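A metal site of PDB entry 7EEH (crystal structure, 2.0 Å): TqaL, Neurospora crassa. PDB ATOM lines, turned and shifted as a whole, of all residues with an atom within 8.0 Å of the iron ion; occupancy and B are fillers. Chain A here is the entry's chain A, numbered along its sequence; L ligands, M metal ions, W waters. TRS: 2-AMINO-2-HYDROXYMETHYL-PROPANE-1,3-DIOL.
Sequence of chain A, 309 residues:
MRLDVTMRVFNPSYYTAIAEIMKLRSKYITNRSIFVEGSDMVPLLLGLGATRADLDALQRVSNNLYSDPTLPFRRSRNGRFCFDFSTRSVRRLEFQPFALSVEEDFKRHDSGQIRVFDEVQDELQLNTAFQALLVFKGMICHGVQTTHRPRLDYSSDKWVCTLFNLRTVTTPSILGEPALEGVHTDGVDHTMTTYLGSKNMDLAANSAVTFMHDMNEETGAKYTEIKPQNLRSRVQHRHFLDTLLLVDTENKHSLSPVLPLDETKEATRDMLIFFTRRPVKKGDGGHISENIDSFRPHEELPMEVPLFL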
ATOM      1  N   GLU A 181      -1.184 -10.458 -16.212  1.00  0.00           N
ATOM      2  CA  GLU A 181      -2.069  -9.493 -15.569  1.00  0.00           C
ATOM      3  C   GLU A 181      -2.660  -8.552 -16.611  1.00  0.00           C
ATOM      4  O   GLU A 181      -1.982  -8.101 -17.532  1.00  0.00           O
ATOM      5  CB  GLU A 181      -1.296  -8.681 -14.522  1.00  0.00           C
ATOM      6  CG  GLU A 181      -1.702  -8.910 -13.059  1.00  0.00           C
ATOM      7  CD  GLU A 181      -1.407  -7.702 -12.166  1.00  0.00           C
ATOM      8  OE1 GLU A 181      -0.210  -7.415 -11.890  1.00  0.00           O
ATOM      9  OE2 GLU A 181      -2.369  -7.024 -11.722  1.00  0.00           O
ATOM     10  N   GLY A 182      -3.951  -8.251 -16.463  1.00  0.00           N
ATOM     11  CA  GLY A 182      -4.634  -7.321 -17.342  1.00  0.00           C
ATOM     12  C   GLY A 182      -4.606  -5.899 -16.809  1.00  0.00           C
ATOM     13  O   GLY A 182      -3.894  -5.575 -15.854  1.00  0.00           O
ATOM     14  N   VAL A 183      -5.405  -5.041 -17.451  1.00  0.00           N
ATOM     15  CA  VAL A 183      -5.516  -3.645 -17.030  1.00  0.00           C
ATOM     16  C   VAL A 183      -5.848  -3.568 -15.536  1.00  0.00           C
ATOM     17  O   VAL A 183      -6.713  -4.295 -15.048  1.00  0.00           O
ATOM     18  CB  VAL A 183      -6.599  -2.953 -17.871  1.00  0.00           C
ATOM     19  CG1 VAL A 183      -6.797  -1.499 -17.419  1.00  0.00           C
ATOM     20  CG2 VAL A 183      -6.217  -3.010 -19.356  1.00  0.00           C
ATOM     21  N   HIS A 184      -5.168  -2.678 -14.819  1.00  0.00           N
ATOM     22  CA  HIS A 184      -5.334  -2.612 -13.364  1.00  0.00           C
ATOM     23  C   HIS A 184      -4.722  -1.326 -12.818  1.00  0.00           C
ATOM     24  O   HIS A 184      -3.981  -0.628 -13.521  1.00  0.00           O
ATOM     25  CB  HIS A 184      -4.686  -3.830 -12.682  1.00  0.00           C
ATOM     26  CG  HIS A 184      -3.192  -3.828 -12.782  1.00  0.00           C
ATOM     27  ND1 HIS A 184      -2.522  -4.259 -13.907  1.00  0.00           N
ATOM     28  CD2 HIS A 184      -2.232  -3.438 -11.910  1.00  0.00           C
ATOM     29  CE1 HIS A 184      -1.222  -4.140 -13.716  1.00  0.00           C
ATOM     30  NE2 HIS A 184      -1.018  -3.639 -12.517  1.00  0.00           N
ATOM     31  N   THR A 185      -5.047  -1.033 -11.559  1.00  0.00           N
ATOM     32  CA  THR A 185      -4.206  -0.246 -10.679  1.00  0.00           C
ATOM     33  C   THR A 185      -3.601  -1.174  -9.630  1.00  0.00           C
ATOM     34  O   THR A 185      -4.114  -2.265  -9.371  1.00  0.00           O
ATOM     35  CB  THR A 185      -4.986   0.915 -10.000  1.00  0.00           C
ATOM     36  OG1 THR A 185      -5.585   0.468  -8.787  1.00  0.00           O
ATOM     37  CG2 THR A 185      -6.059   1.477 -10.903  1.00  0.00           C
ATOM     38  N   ASP A 186      -2.462  -0.737  -9.068  1.00  0.00           N
ATOM     39  CA  ASP A 186      -1.729  -1.476  -8.042  1.00  0.00           C
ATOM     40  C   ASP A 186      -2.285  -1.271  -6.637  1.00  0.00           C
ATOM     41  O   ASP A 186      -1.704  -1.799  -5.681  1.00  0.00           O
ATOM     42  CB  ASP A 186      -0.245  -1.069  -8.048  1.00  0.00           C
ATOM     43  CG  ASP A 186       0.413  -1.177  -9.430  1.00  0.00           C
ATOM     44  OD1 ASP A 186       0.093  -2.127 -10.183  1.00  0.00           O
ATOM     45  OD2 ASP A 186       1.286  -0.325  -9.736  1.00  0.00           O
ATOM     46  N   GLY A 187      -3.356  -0.501  -6.493  1.00  0.00           N
ATOM     47  CA  GLY A 187      -3.939  -0.242  -5.191  1.00  0.00           C
ATOM     48  C   GLY A 187      -3.152   0.673  -4.275  1.00  0.00           C
ATOM     49  O   GLY A 187      -3.331   0.608  -3.059  1.00  0.00           O
ATOM     50  N   THR A 191       3.226   4.742  -8.108  1.00  0.00           N
ATOM     51  CA  THR A 191       4.060   3.616  -8.505  1.00  0.00           C
ATOM     52  C   THR A 191       5.240   4.103  -9.343  1.00  0.00           C
ATOM     53  O   THR A 191       5.072   4.910 -10.270  1.00  0.00           O
ATOM     54  CB  THR A 191       3.251   2.587  -9.316  1.00  0.00           C
ATOM     55  OG1 THR A 191       2.159   2.099  -8.527  1.00  0.00           O
ATOM     56  CG2 THR A 191       4.133   1.381  -9.740  1.00  0.00           C
ATOM     57  N   THR A 193       8.661   2.497 -11.505  1.00  0.00           N
ATOM     58  CA  THR A 193       9.364   1.350 -12.065  1.00  0.00           C
ATOM     59  C   THR A 193      10.649   1.848 -12.729  1.00  0.00           C
ATOM     60  O   THR A 193      10.598   2.684 -13.646  1.00  0.00           O
ATOM     61  CB  THR A 193       8.475   0.584 -13.060  1.00  0.00           C
ATOM     62  OG1 THR A 193       8.081   1.433 -14.141  1.00  0.00           O
ATOM     63  CG2 THR A 193       7.219   0.073 -12.369  1.00  0.00           C
ATOM     64  N   THR A 210       4.814  -0.776 -21.290  1.00  0.00           N
ATOM     65  CA  THR A 210       3.815  -0.385 -20.284  1.00  0.00           C
ATOM     66  C   THR A 210       2.770   0.515 -20.957  1.00  0.00           C
ATOM     67  O   THR A 210       3.086   1.619 -21.400  1.00  0.00           O
ATOM     68  CB  THR A 210       4.442   0.323 -19.081  1.00  0.00           C
ATOM     69  OG1 THR A 210       5.449  -0.505 -18.466  1.00  0.00           O
ATOM     70  CG2 THR A 210       3.344   0.622 -18.029  1.00  0.00           C
ATOM     71  N   LEU A 246       3.970   7.037 -11.917  1.00  0.00           N
ATOM     72  CA  LEU A 246       2.574   7.233 -12.275  1.00  0.00           C
ATOM     73  C   LEU A 246       1.704   7.343 -11.030  1.00  0.00           C
ATOM     74  O   LEU A 246       1.944   6.675 -10.016  1.00  0.00           O
ATOM     75  CB  LEU A 246       2.059   6.107 -13.182  1.00  0.00           C
ATOM     76  CG  LEU A 246       1.973   4.657 -12.711  1.00  0.00           C
ATOM     77  CD1 LEU A 246       0.629   4.379 -12.054  1.00  0.00           C
ATOM     78  CD2 LEU A 246       2.161   3.701 -13.881  1.00  0.00           C
ATOM     79  N   ASP A 248      -1.201   6.189  -9.229  1.00  0.00           N
ATOM     80  CA  ASP A 248      -1.852   4.897  -9.381  1.00  0.00           C
ATOM     81  C   ASP A 248      -3.364   4.976  -9.224  1.00  0.00           C
ATOM     82  O   ASP A 248      -4.070   4.099  -9.720  1.00  0.00           O
ATOM     83  CB  ASP A 248      -1.259   3.915  -8.381  1.00  0.00           C
ATOM     84  CG  ASP A 248      -1.810   2.495  -8.544  1.00  0.00           C
ATOM     85  OD1 ASP A 248      -1.793   1.972  -9.672  1.00  0.00           O
ATOM     86  OD2 ASP A 248      -2.246   1.906  -7.521  1.00  0.00           O
ATOM     87  N   LYS A 252      -4.872   3.730 -15.189  1.00  0.00           N
ATOM     88  CA  LYS A 252      -4.761   2.283 -15.151  1.00  0.00           C
ATOM     89  C   LYS A 252      -3.604   1.921 -16.061  1.00  0.00           C
ATOM     90  O   LYS A 252      -3.210   2.711 -16.920  1.00  0.00           O
ATOM     91  CB  LYS A 252      -6.056   1.594 -15.607  1.00  0.00           C
ATOM     92  CG  LYS A 252      -7.171   1.616 -14.553  1.00  0.00           C
ATOM     93  CD  LYS A 252      -8.444   0.906 -15.039  1.00  0.00           C
ATOM     94  CE  LYS A 252      -9.697   1.591 -14.455  1.00  0.00           C
ATOM     95  NZ  LYS A 252     -10.997   0.878 -14.714  1.00  0.00           N
ATOM     96  N   HIS A 253      -3.039   0.729 -15.858  1.00  0.00           N
ATOM     97  CA  HIS A 253      -1.881   0.332 -16.647  1.00  0.00           C
ATOM     98  C   HIS A 253      -1.881  -1.177 -16.904  1.00  0.00           C
ATOM     99  O   HIS A 253      -2.572  -1.953 -16.237  1.00  0.00           O
ATOM    100  CB  HIS A 253      -0.564   0.762 -15.959  1.00  0.00           C
ATOM    101  CG  HIS A 253      -0.351   0.178 -14.600  1.00  0.00           C
ATOM    102  ND1 HIS A 253      -0.975   0.667 -13.469  1.00  0.00           N
ATOM    103  CD2 HIS A 253       0.443  -0.844 -14.182  1.00  0.00           C
ATOM    104  CE1 HIS A 253      -0.578  -0.031 -12.416  1.00  0.00           C
ATOM    105  NE2 HIS A 253       0.278  -0.945 -12.820  1.00  0.00           N
ATOM    106  N   SER A 254      -1.078  -1.573 -17.895  1.00  0.00           N
ATOM    107  CA  SER A 254      -0.818  -2.988 -18.169  1.00  0.00           C
ATOM    108  C   SER A 254       0.585  -3.078 -18.747  1.00  0.00           C
ATOM    109  O   SER A 254       1.084  -2.108 -19.318  1.00  0.00           O
ATOM    110  CB  SER A 254      -1.839  -3.578 -19.152  1.00  0.00           C
ATOM    111  OG  SER A 254      -1.792  -2.896 -20.397  1.00  0.00           O
ATOM    112  N   LEU A 255       1.212  -4.254 -18.576  1.00  0.00           N
ATOM    113  CA  LEU A 255       2.580  -4.508 -19.011  1.00  0.00           C
ATOM    114  C   LEU A 255       2.605  -5.769 -19.854  1.00  0.00           C
ATOM    115  O   LEU A 255       2.238  -6.852 -19.378  1.00  0.00           O
ATOM    116  CB  LEU A 255       3.523  -4.671 -17.805  1.00  0.00           C
ATOM    117  CG  LEU A 255       5.009  -4.974 -18.121  1.00  0.00           C
ATOM    118  CD1 LEU A 255       5.761  -3.751 -18.651  1.00  0.00           C
ATOM    119  CD2 LEU A 255       5.794  -5.603 -16.946  1.00  0.00           C
ATOM    120  N   ILE A 273      10.715  -1.878  -8.466  1.00  0.00           N
ATOM    121  CA  ILE A 273       9.307  -1.474  -8.478  1.00  0.00           C
ATOM    122  C   ILE A 273       8.982  -0.927  -7.094  1.00  0.00           C
ATOM    123  O   ILE A 273       9.055  -1.657  -6.102  1.00  0.00           O
ATOM    124  CB  ILE A 273       8.371  -2.645  -8.847  1.00  0.00           C
ATOM    125  CG1 ILE A 273       8.817  -3.335 -10.144  1.00  0.00           C
ATOM    126  CG2 ILE A 273       6.942  -2.168  -8.954  1.00  0.00           C
ATOM    127  CD1 ILE A 273       8.280  -4.768 -10.285  1.00  0.00           C
ATOM    128  N   PHE A 275       6.145   0.728  -4.724  1.00  0.00           N
ATOM    129  CA  PHE A 275       4.704   0.904  -4.512  1.00  0.00           C
ATOM    130  C   PHE A 275       4.516   1.753  -3.260  1.00  0.00           C
ATOM    131  O   PHE A 275       4.744   1.270  -2.141  1.00  0.00           O
ATOM    132  CB  PHE A 275       3.989  -0.421  -4.316  1.00  0.00           C
ATOM    133  CG  PHE A 275       4.078  -1.387  -5.475  1.00  0.00           C
ATOM    134  CD1 PHE A 275       3.372  -1.151  -6.646  1.00  0.00           C
ATOM    135  CD2 PHE A 275       4.763  -2.592  -5.336  1.00  0.00           C
ATOM    136  CE1 PHE A 275       3.409  -2.079  -7.694  1.00  0.00           C
ATOM    137  CE2 PHE A 275       4.791  -3.514  -6.375  1.00  0.00           C
ATOM    138  CZ  PHE A 275       4.114  -3.264  -7.545  1.00  0.00           C
HETATM  139  C   TRS L   1       3.779  -2.717 -12.782  1.00  0.00           C
HETATM  140  C1  TRS L   1       3.890  -1.795 -13.994  1.00  0.00           C
HETATM  141  C2  TRS L   1       3.057  -3.966 -13.244  1.00  0.00           C
HETATM  142  C3  TRS L   1       5.180  -3.153 -12.362  1.00  0.00           C
HETATM  143  N   TRS L   1       3.091  -2.056 -11.650  1.00  0.00           N
HETATM  144  O1  TRS L   1       3.855  -0.437 -13.592  1.00  0.00           O
HETATM  145  O2  TRS L   1       1.725  -3.654 -13.598  1.00  0.00           O
HETATM  146  O3  TRS L   1       5.766  -3.814 -13.471  1.00  0.00           O
HETATM  147 FE    FE M   1       0.900  -2.827 -11.975  1.00  0.00          FE
HETATM  148  O   HOH W   1       1.317  -4.575 -10.847  1.00  0.00           O
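The side-chain hydroxyl (OG1) of Thr 191 lies within hydrogen-bond range of the side-chain carboxylate (OD2) of Asp 186. The backbone NH (N) of Asp 186 lies within hydrogen-bond range of the side-chain carboxylate (OD1) of Asp 248 (2.9 Å). ND1 of His 184 sits at hydrogen-bond distance from O of Gly 182 (2.7 Å).
Of the 18 residues printed, 3 come within 4 Å of the iron ion.
The iron ion is bound by an oxygen (O2) of the ligand (2.0 Å), the side-chain carboxylate of Asp 186 (2.1 Å), water W1 (2.1 Å), a ring nitrogen (NE2) of His 184 (2.2 Å), a ring nitrogen (NE2) of His 253 (2.2 Å) and a nitrogen (N) of the ligand (2.3 Å).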
